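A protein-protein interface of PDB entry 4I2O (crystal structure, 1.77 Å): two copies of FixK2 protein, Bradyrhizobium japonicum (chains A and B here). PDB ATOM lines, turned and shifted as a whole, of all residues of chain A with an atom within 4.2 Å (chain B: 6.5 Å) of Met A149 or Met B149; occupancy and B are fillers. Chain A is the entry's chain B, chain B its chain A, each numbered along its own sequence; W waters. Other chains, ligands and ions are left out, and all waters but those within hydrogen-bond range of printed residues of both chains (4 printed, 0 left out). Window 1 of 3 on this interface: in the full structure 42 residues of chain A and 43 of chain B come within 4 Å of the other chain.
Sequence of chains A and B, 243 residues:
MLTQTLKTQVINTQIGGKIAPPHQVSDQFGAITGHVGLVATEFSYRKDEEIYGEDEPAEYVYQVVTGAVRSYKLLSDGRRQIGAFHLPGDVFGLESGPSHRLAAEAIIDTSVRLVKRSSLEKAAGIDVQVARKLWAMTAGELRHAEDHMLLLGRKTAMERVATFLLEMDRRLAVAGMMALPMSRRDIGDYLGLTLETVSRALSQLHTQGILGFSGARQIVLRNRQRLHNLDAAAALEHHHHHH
Gln A81 touches Gly B153, and with the chains exchanged Gly A153 touches Gln B81. Ala A145 touches Met B149, and with the chains exchanged Met A149 touches Ala B145. Met A149 touches Leu B152, and with the chains exchanged Leu A152 touches Met B149. Leu A152 touches Gly B153, but with the chains exchanged Gly A153 does not touch Leu B152 (4.03 Å). Of the 18 pairs that touch across the chains among the printed residues, 15 have their exchanged pair printed and touching as well.
Of the printed residues of chain B, His A148 touches Met B149. Of chain B, only Gln B81 (3.7 Å), Ala B145 (3.9 Å), His B148 (3.8 Å), Met B149 (3.7 Å) and Leu B152 (3.5 Å) come within 4 Å of Met A149. Printed residues of chain B within 4 Å of Leu A152: Met B149 (3.5 Å), Leu B152 (3.5 Å) and Gly B153 (3.99 Å). Ala B84 touches none of the printed residues of chain A. Met B149 touches five residues of chain A. Leu B151 touches none of the printed residues of chain A.
Water W4 lies within hydrogen-bond range of ND1 of His B144 (2.6 Å), O of Gly B83 (2.8 Å), N of Ala B145 (3.4 Å) and SD of Met A149 (3.7 Å). Water W1 lies within hydrogen-bond range of the backbone carbonyl oxygen (O) of Leu A152 (2.8 Å) and the backbone carbonyl oxygen (O) of Leu B152 (3.2 Å). Water W2 bridges O of Leu B152 (2.9 Å) and O of Leu A152 (3.3 Å). Water W3 bridges the backbone NH (N) of Ala A145 and the side-chain sulfur (SD) of Met B149.
Among the printed residues, merely in contact across the chains: Gln A81 with Gly B153 (3.2 Å), Glu A146 with Leu B102 (3.2 Å), Gly A153 with Gln B81 (3.2 Å), Met A149 with Leu B152 (3.5 Å), Leu A152 with Met B149 (3.5 Å), Leu A152 with Leu B152 (3.5 Å), Ala A145 with Met B149 (3.6 Å), Leu A150 with Gln B81 (3.6 Å), Gln A81 with Leu B150 (3.6 Å), Met A149 with Gln B81 (3.7 Å), Gln A81 with Met B149 (3.7 Å), Ala A145 with Ala B145 (3.7 Å), Met A149 with Met B149 (3.7 Å), Met A149 with His B148 (3.8 Å), His A148 with Met B149 (3.8 Å), Gln A81 with Arg B154 (3.9 Å), Met A149 with Ala B145 (3.9 Å) and Leu A152 with Gly B153 (3.99 Å).
Hydrophobic or aromatic side chains of chain B that line the printed part of chain A: Leu B102, Ala B145, His B148, Met B149, Leu B150 and Leu B152. Along chain B the printed residues that touch a printed residue of chain A span positions 81 to 154. Hydrophobic or aromatic side chains of chain A within 4 Å of the printed part of chain B: Ala A145, His A148, Met A149, Leu A150 and Leu A152. Among the printed residues, no Asp or Glu carboxylate lies within 4 Å of a Lys or Arg side-chain nitrogen of the other chain.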
ATOM      1  N   GLN A  81      -7.398  -6.153 -15.520  1.00  0.00           N
ATOM      2  CA  GLN A  81      -6.018  -5.906 -15.895  1.00  0.00           C
ATOM      3  C   GLN A  81      -6.011  -4.567 -16.618  1.00  0.00           C
ATOM      4  O   GLN A  81      -6.677  -4.408 -17.676  1.00  0.00           O
ATOM      5  CB  GLN A  81      -5.484  -7.052 -16.815  1.00  0.00           C
ATOM      6  CG  GLN A  81      -4.059  -6.771 -17.288  1.00  0.00           C
ATOM      7  CD  GLN A  81      -3.071  -6.723 -16.157  1.00  0.00           C
ATOM      8  OE1 GLN A  81      -3.080  -7.621 -15.277  1.00  0.00           O
ATOM      9  NE2 GLN A  81      -2.162  -5.731 -16.178  1.00  0.00           N
ATOM     10  N   ALA A 145       3.615  -3.872 -24.458  1.00  0.00           N
ATOM     11  CA  ALA A 145       2.860  -5.045 -23.992  1.00  0.00           C
ATOM     12  C   ALA A 145       3.778  -6.234 -23.776  1.00  0.00           C
ATOM     13  O   ALA A 145       3.590  -6.988 -22.782  1.00  0.00           O
ATOM     14  CB  ALA A 145       1.680  -5.451 -24.987  1.00  0.00           C
ATOM     15  N   GLU A 146       4.738  -6.391 -24.674  1.00  0.00           N
ATOM     16  CA  GLU A 146       5.770  -7.484 -24.538  1.00  0.00           C
ATOM     17  C   GLU A 146       6.569  -7.344 -23.237  1.00  0.00           C
ATOM     18  O   GLU A 146       6.727  -8.289 -22.434  1.00  0.00           O
ATOM     19  CB  GLU A 146       6.733  -7.473 -25.735  1.00  0.00           C
ATOM     20  CG  GLU A 146       6.029  -7.920 -27.033  1.00  0.00           C
ATOM     21  CD  GLU A 146       6.833  -7.700 -28.312  1.00  0.00           C
ATOM     22  OE1 GLU A 146       7.784  -6.882 -28.341  1.00  0.00           O
ATOM     23  OE2 GLU A 146       6.539  -8.390 -29.328  1.00  0.00           O
ATOM     24  N   ASP A 147       7.072  -6.140 -22.990  1.00  0.00           N
ATOM     25  CA  ASP A 147       7.740  -5.891 -21.680  1.00  0.00           C
ATOM     26  C   ASP A 147       6.791  -6.124 -20.524  1.00  0.00           C
ATOM     27  O   ASP A 147       7.194  -6.640 -19.440  1.00  0.00           O
ATOM     28  CB  ASP A 147       8.200  -4.413 -21.595  1.00  0.00           C
ATOM     29  CG  ASP A 147       9.365  -4.092 -22.511  1.00  0.00           C
ATOM     30  OD1 ASP A 147      10.042  -5.010 -23.011  1.00  0.00           O
ATOM     31  OD2 ASP A 147       9.633  -2.884 -22.715  1.00  0.00           O
ATOM     32  N   HIS A 148       5.522  -5.717 -20.707  1.00  0.00           N
ATOM     33  CA  HIS A 148       4.579  -5.840 -19.613  1.00  0.00           C
ATOM     34  C   HIS A 148       4.199  -7.320 -19.387  1.00  0.00           C
ATOM     35  O   HIS A 148       3.970  -7.743 -18.215  1.00  0.00           O
ATOM     36  CB  HIS A 148       3.344  -4.976 -19.832  1.00  0.00           C
ATOM     37  CG  HIS A 148       2.780  -4.444 -18.557  1.00  0.00           C
ATOM     38  ND1 HIS A 148       3.550  -3.784 -17.629  1.00  0.00           N
ATOM     39  CD2 HIS A 148       1.525  -4.496 -18.062  1.00  0.00           C
ATOM     40  CE1 HIS A 148       2.785  -3.450 -16.593  1.00  0.00           C
ATOM     41  NE2 HIS A 148       1.554  -3.888 -16.831  1.00  0.00           N
ATOM     42  N   MET A 149       4.185  -8.134 -20.441  1.00  0.00           N
ATOM     43  CA  MET A 149       4.002  -9.588 -20.165  1.00  0.00           C
ATOM     44  C   MET A 149       5.109 -10.182 -19.295  1.00  0.00           C
ATOM     45  O   MET A 149       4.876 -11.058 -18.425  1.00  0.00           O
ATOM     46  CB  MET A 149       3.935 -10.367 -21.496  1.00  0.00           C
ATOM     47  CG  MET A 149       2.615 -10.116 -22.244  1.00  0.00           C
ATOM     48  SD  MET A 149       2.502 -11.136 -23.734  1.00  0.00           S
ATOM     49  CE  MET A 149       3.873 -10.555 -24.707  1.00  0.00           C
ATOM     50  N   LEU A 150       6.348  -9.764 -19.545  1.00  0.00           N
ATOM     51  CA  LEU A 150       7.446 -10.265 -18.737  1.00  0.00           C
ATOM     52  C   LEU A 150       7.255  -9.845 -17.282  1.00  0.00           C
ATOM     53  O   LEU A 150       7.520 -10.604 -16.335  1.00  0.00           O
ATOM     54  CB  LEU A 150       8.761  -9.759 -19.280  1.00  0.00           C
ATOM     55  CG  LEU A 150      10.037 -10.054 -18.520  1.00  0.00           C
ATOM     56  CD1 LEU A 150      10.337 -11.592 -18.420  1.00  0.00           C
ATOM     57  CD2 LEU A 150      11.243  -9.324 -19.149  1.00  0.00           C
ATOM     58  N   LEU A 151       6.827  -8.613 -17.081  1.00  0.00           N
ATOM     59  CA  LEU A 151       6.567  -8.157 -15.701  1.00  0.00           C
ATOM     60  C   LEU A 151       5.475  -8.962 -15.026  1.00  0.00           C
ATOM     61  O   LEU A 151       5.658  -9.424 -13.863  1.00  0.00           O
ATOM     62  CB  LEU A 151       6.162  -6.630 -15.809  1.00  0.00           C
ATOM     63  CG  LEU A 151       5.775  -5.955 -14.447  1.00  0.00           C
ATOM     64  CD1 LEU A 151       6.051  -4.439 -14.567  1.00  0.00           C
ATOM     65  CD2 LEU A 151       4.274  -6.107 -14.006  1.00  0.00           C
ATOM     66  N   LEU A 152       4.350  -9.180 -15.704  1.00  0.00           N
ATOM     67  CA  LEU A 152       3.190  -9.866 -15.135  1.00  0.00           C
ATOM     68  C   LEU A 152       3.445 -11.370 -14.995  1.00  0.00           C
ATOM     69  O   LEU A 152       2.939 -12.000 -14.027  1.00  0.00           O
ATOM     70  CB  LEU A 152       1.922  -9.667 -15.965  1.00  0.00           C
ATOM     71  CG  LEU A 152       1.459  -8.174 -16.091  1.00  0.00           C
ATOM     72  CD1 LEU A 152       0.427  -8.099 -17.226  1.00  0.00           C
ATOM     73  CD2 LEU A 152       0.840  -7.770 -14.767  1.00  0.00           C
ATOM     74  N   GLY A 153       4.249 -11.939 -15.887  1.00  0.00           N
ATOM     75  CA  GLY A 153       4.506 -13.367 -15.749  1.00  0.00           C
ATOM     76  C   GLY A 153       5.655 -13.707 -14.821  1.00  0.00           C
ATOM     77  O   GLY A 153       5.678 -14.788 -14.169  1.00  0.00           O
ATOM     78  N   GLN B  81       9.898 -15.458 -19.799  1.00  0.00           N
ATOM     79  CA  GLN B  81       8.509 -15.323 -20.185  1.00  0.00           C
ATOM     80  C   GLN B  81       8.488 -15.634 -21.669  1.00  0.00           C
ATOM     81  O   GLN B  81       9.152 -14.929 -22.480  1.00  0.00           O
ATOM     82  CB  GLN B  81       7.972 -13.881 -19.918  1.00  0.00           C
ATOM     83  CG  GLN B  81       6.558 -13.737 -20.480  1.00  0.00           C
ATOM     84  CD  GLN B  81       5.555 -14.595 -19.767  1.00  0.00           C
ATOM     85  OE1 GLN B  81       5.561 -14.677 -18.511  1.00  0.00           O
ATOM     86  NE2 GLN B  81       4.619 -15.195 -20.542  1.00  0.00           N
ATOM     87  N   ILE B  82       7.774 -16.706 -22.044  1.00  0.00           N
ATOM     88  CA  ILE B  82       7.480 -16.913 -23.477  1.00  0.00           C
ATOM     89  C   ILE B  82       6.261 -16.043 -23.900  1.00  0.00           C
ATOM     90  O   ILE B  82       5.123 -16.154 -23.337  1.00  0.00           O
ATOM     91  CB  ILE B  82       7.229 -18.426 -23.712  1.00  0.00           C
ATOM     92  CG1 ILE B  82       8.571 -19.147 -23.621  1.00  0.00           C
ATOM     93  CG2 ILE B  82       6.675 -18.605 -25.155  1.00  0.00           C
ATOM     94  CD1 ILE B  82       8.440 -20.713 -23.645  1.00  0.00           C
ATOM     95  N   GLY B  83       6.455 -15.184 -24.914  1.00  0.00           N
ATOM     96  CA  GLY B  83       5.428 -14.284 -25.367  1.00  0.00           C
ATOM     97  C   GLY B  83       4.544 -14.912 -26.403  1.00  0.00           C
ATOM     98  O   GLY B  83       3.360 -14.543 -26.521  1.00  0.00           O
ATOM     99  N   ALA B  84       5.067 -15.924 -27.126  1.00  0.00           N
ATOM    100  CA  ALA B  84       4.256 -16.517 -28.150  1.00  0.00           C
ATOM    101  C   ALA B  84       4.895 -17.812 -28.627  1.00  0.00           C
ATOM    102  O   ALA B  84       6.126 -17.952 -28.599  1.00  0.00           O
ATOM    103  CB  ALA B  84       4.112 -15.546 -29.389  1.00  0.00           C
ATOM    104  N   LEU B 102      12.171  -9.693 -28.924  1.00  0.00           N
ATOM    105  CA  LEU B 102      12.144 -10.967 -28.249  1.00  0.00           C
ATOM    106  C   LEU B 102      13.173 -11.844 -28.968  1.00  0.00           C
ATOM    107  O   LEU B 102      13.441 -11.635 -30.148  1.00  0.00           O
ATOM    108  CB  LEU B 102      10.762 -11.656 -28.347  1.00  0.00           C
ATOM    109  CG  LEU B 102       9.735 -11.159 -27.294  1.00  0.00           C
ATOM    110  CD1 LEU B 102       9.173  -9.847 -27.727  1.00  0.00           C
ATOM    111  CD2 LEU B 102       8.599 -12.101 -27.030  1.00  0.00           C
ATOM    112  N   LEU B 142      -0.279  -7.564 -31.232  1.00  0.00           N
ATOM    113  CA  LEU B 142      -0.720  -6.732 -30.117  1.00  0.00           C
ATOM    114  C   LEU B 142      -2.005  -7.288 -29.441  1.00  0.00           C
ATOM    115  O   LEU B 142      -2.110  -7.310 -28.172  1.00  0.00           O
ATOM    116  CB  LEU B 142      -0.909  -5.294 -30.598  1.00  0.00           C
ATOM    117  CG  LEU B 142      -1.432  -4.304 -29.526  1.00  0.00           C
ATOM    118  CD1 LEU B 142      -0.501  -4.167 -28.295  1.00  0.00           C
ATOM    119  CD2 LEU B 142      -1.670  -2.912 -30.187  1.00  0.00           C
ATOM    120  N   HIS B 144      -2.999 -10.368 -29.424  1.00  0.00           N
ATOM    121  CA  HIS B 144      -2.597 -11.540 -28.633  1.00  0.00           C
ATOM    122  C   HIS B 144      -1.927 -11.163 -27.294  1.00  0.00           C
ATOM    123  O   HIS B 144      -2.247 -11.769 -26.264  1.00  0.00           O
ATOM    124  CB  HIS B 144      -1.651 -12.414 -29.466  1.00  0.00           C
ATOM    125  CG  HIS B 144      -1.428 -13.788 -28.888  1.00  0.00           C
ATOM    126  ND1 HIS B 144      -0.484 -14.022 -27.927  1.00  0.00           N
ATOM    127  CD2 HIS B 144      -2.015 -14.986 -29.161  1.00  0.00           C
ATOM    128  CE1 HIS B 144      -0.519 -15.324 -27.584  1.00  0.00           C
ATOM    129  NE2 HIS B 144      -1.426 -15.921 -28.329  1.00  0.00           N
ATOM    130  N   ALA B 145      -1.043 -10.155 -27.307  1.00  0.00           N
ATOM    131  CA  ALA B 145      -0.296  -9.752 -26.133  1.00  0.00           C
ATOM    132  C   ALA B 145      -1.244  -9.118 -25.130  1.00  0.00           C
ATOM    133  O   ALA B 145      -1.084  -9.370 -23.913  1.00  0.00           O
ATOM    134  CB  ALA B 145       0.885  -8.763 -26.501  1.00  0.00           C
ATOM    135  N   GLU B 146      -2.207  -8.327 -25.603  1.00  0.00           N
ATOM    136  CA  GLU B 146      -3.240  -7.747 -24.682  1.00  0.00           C
ATOM    137  C   GLU B 146      -4.030  -8.823 -23.937  1.00  0.00           C
ATOM    138  O   GLU B 146      -4.208  -8.784 -22.692  1.00  0.00           O
ATOM    139  CB  GLU B 146      -4.205  -6.822 -25.456  1.00  0.00           C
ATOM    140  CG  GLU B 146      -3.505  -5.520 -25.940  1.00  0.00           C
ATOM    141  CD  GLU B 146      -4.300  -4.720 -26.963  1.00  0.00           C
ATOM    142  OE1 GLU B 146      -5.229  -5.266 -27.627  1.00  0.00           O
ATOM    143  OE2 GLU B 146      -4.022  -3.498 -27.077  1.00  0.00           O
ATOM    144  N   ASP B 147      -4.499  -9.813 -24.671  1.00  0.00           N
ATOM    145  CA  ASP B 147      -5.211 -10.922 -24.028  1.00  0.00           C
ATOM    146  C   ASP B 147      -4.278 -11.622 -23.081  1.00  0.00           C
ATOM    147  O   ASP B 147      -4.706 -12.061 -21.973  1.00  0.00           O
ATOM    148  CB  ASP B 147      -5.690 -11.951 -25.097  1.00  0.00           C
ATOM    149  CG  ASP B 147      -6.871 -11.455 -25.917  1.00  0.00           C
ATOM    150  OD1 ASP B 147      -7.530 -10.462 -25.522  1.00  0.00           O
ATOM    151  OD2 ASP B 147      -7.166 -12.092 -26.965  1.00  0.00           O
ATOM    152  N   HIS B 148      -3.012 -11.816 -23.514  1.00  0.00           N
ATOM    153  CA  HIS B 148      -2.065 -12.543 -22.675  1.00  0.00           C
ATOM    154  C   HIS B 148      -1.698 -11.745 -21.418  1.00  0.00           C
ATOM    155  O   HIS B 148      -1.469 -12.343 -20.362  1.00  0.00           O
ATOM    156  CB  HIS B 148      -0.812 -12.925 -23.424  1.00  0.00           C
ATOM    157  CG  HIS B 148      -0.295 -14.245 -23.035  1.00  0.00           C
ATOM    158  ND1 HIS B 148      -1.086 -15.389 -22.999  1.00  0.00           N
ATOM    159  CD2 HIS B 148       0.945 -14.628 -22.665  1.00  0.00           C
ATOM    160  CE1 HIS B 148      -0.357 -16.390 -22.554  1.00  0.00           C
ATOM    161  NE2 HIS B 148       0.890 -15.963 -22.365  1.00  0.00           N
ATOM    162  N   MET B 149      -1.668 -10.414 -21.475  1.00  0.00           N
ATOM    163  CA  MET B 149      -1.513  -9.687 -20.186  1.00  0.00           C
ATOM    164  C   MET B 149      -2.602  -9.944 -19.199  1.00  0.00           C
ATOM    165  O   MET B 149      -2.351 -10.047 -17.975  1.00  0.00           O
ATOM    166  CB  MET B 149      -1.418  -8.167 -20.460  1.00  0.00           C
ATOM    167  CG  MET B 149      -0.110  -7.782 -21.174  1.00  0.00           C
ATOM    168  SD  MET B 149       0.016  -5.949 -21.357  1.00  0.00           S
ATOM    169  CE  MET B 149      -1.063  -5.536 -22.691  1.00  0.00           C
ATOM    170  N   LEU B 150      -3.850  -9.990 -19.679  1.00  0.00           N
ATOM    171  CA  LEU B 150      -4.971 -10.296 -18.798  1.00  0.00           C
ATOM    172  C   LEU B 150      -4.754 -11.651 -18.161  1.00  0.00           C
ATOM    173  O   LEU B 150      -5.013 -11.854 -16.984  1.00  0.00           O
ATOM    174  CB  LEU B 150      -6.288 -10.274 -19.562  1.00  0.00           C
ATOM    175  CG  LEU B 150      -7.584 -10.627 -18.823  1.00  0.00           C
ATOM    176  CD1 LEU B 150      -7.835  -9.697 -17.618  1.00  0.00           C
ATOM    177  CD2 LEU B 150      -8.794 -10.627 -19.750  1.00  0.00           C
ATOM    178  N   LEU B 151      -4.394 -12.634 -18.973  1.00  0.00           N
ATOM    179  CA  LEU B 151      -4.089 -13.959 -18.406  1.00  0.00           C
ATOM    180  C   LEU B 151      -2.997 -13.936 -17.351  1.00  0.00           C
ATOM    181  O   LEU B 151      -3.166 -14.529 -16.247  1.00  0.00           O
ATOM    182  CB  LEU B 151      -3.647 -14.877 -19.616  1.00  0.00           C
ATOM    183  CG  LEU B 151      -3.308 -16.352 -19.200  1.00  0.00           C
ATOM    184  CD1 LEU B 151      -3.633 -17.276 -20.348  1.00  0.00           C
ATOM    185  CD2 LEU B 151      -1.778 -16.582 -18.815  1.00  0.00           C
ATOM    186  N   LEU B 152      -1.865 -13.294 -17.633  1.00  0.00           N
ATOM    187  CA  LEU B 152      -0.714 -13.280 -16.721  1.00  0.00           C
ATOM    188  C   LEU B 152      -0.968 -12.413 -15.484  1.00  0.00           C
ATOM    189  O   LEU B 152      -0.475 -12.753 -14.388  1.00  0.00           O
ATOM    190  CB  LEU B 152       0.567 -12.784 -17.392  1.00  0.00           C
ATOM    191  CG  LEU B 152       1.013 -13.637 -18.618  1.00  0.00           C
ATOM    192  CD1 LEU B 152       2.076 -12.853 -19.393  1.00  0.00           C
ATOM    193  CD2 LEU B 152       1.645 -14.974 -18.089  1.00  0.00           C
ATOM    194  N   GLY B 153      -1.746 -11.367 -15.640  1.00  0.00           N
ATOM    195  CA  GLY B 153      -2.047 -10.511 -14.474  1.00  0.00           C
ATOM    196  C   GLY B 153      -3.170 -11.037 -13.601  1.00  0.00           C
ATOM    197  O   GLY B 153      -3.183 -10.804 -12.366  1.00  0.00           O
ATOM    198  N   ARG B 154      -4.161 -11.709 -14.190  1.00  0.00           N
ATOM    199  CA  ARG B 154      -5.396 -11.898 -13.445  1.00  0.00           C
ATOM    200  C   ARG B 154      -5.978 -13.336 -13.392  1.00  0.00           C
ATOM    201  O   ARG B 154      -6.834 -13.597 -12.509  1.00  0.00           O
ATOM    202  CB  ARG B 154      -6.488 -10.893 -13.929  1.00  0.00           C
ATOM    203  CG  ARG B 154      -6.070  -9.447 -13.657  1.00  0.00           C
ATOM    204  CD  ARG B 154      -6.323  -9.236 -12.163  1.00  0.00           C
ATOM    205  NE  ARG B 154      -5.874  -7.962 -11.528  1.00  0.00           N
ATOM    206  CZ  ARG B 154      -4.943  -7.908 -10.566  1.00  0.00           C
ATOM    207  NH1 ARG B 154      -4.252  -9.000 -10.238  1.00  0.00           N
ATOM    208  NH2 ARG B 154      -4.722  -6.767  -9.898  1.00  0.00           N
ATOM    209  N   LYS B 155      -5.533 -14.281 -14.268  1.00  0.00           N
ATOM    210  CA  LYS B 155      -6.207 -15.589 -14.316  1.00  0.00           C
ATOM    211  C   LYS B 155      -5.597 -16.564 -13.294  1.00  0.00           C
ATOM    212  O   LYS B 155      -4.421 -16.444 -12.931  1.00  0.00           O
ATOM    213  CB  LYS B 155      -6.177 -16.248 -15.753  1.00  0.00           C
ATOM    214  CG  LYS B 155      -7.192 -15.560 -16.670  1.00  0.00           C
ATOM    215  CD  LYS B 155      -7.230 -16.289 -18.050  1.00  0.00           C
ATOM    216  CE  LYS B 155      -8.271 -15.606 -18.969  1.00  0.00           C
ATOM    217  NZ  LYS B 155      -8.426 -16.440 -20.266  1.00  0.00           N
HETATM  218  O   HOH W   1       1.964 -14.551 -13.274  1.00  0.00           O
HETATM  219  O   HOH W   2       0.497 -11.633 -11.909  1.00  0.00           O
HETATM  220  O   HOH W   3       1.076  -2.603 -22.424  1.00  0.00           O
HETATM  221  O   HOH W   4       1.462 -12.496 -26.981  1.00  0.00           O
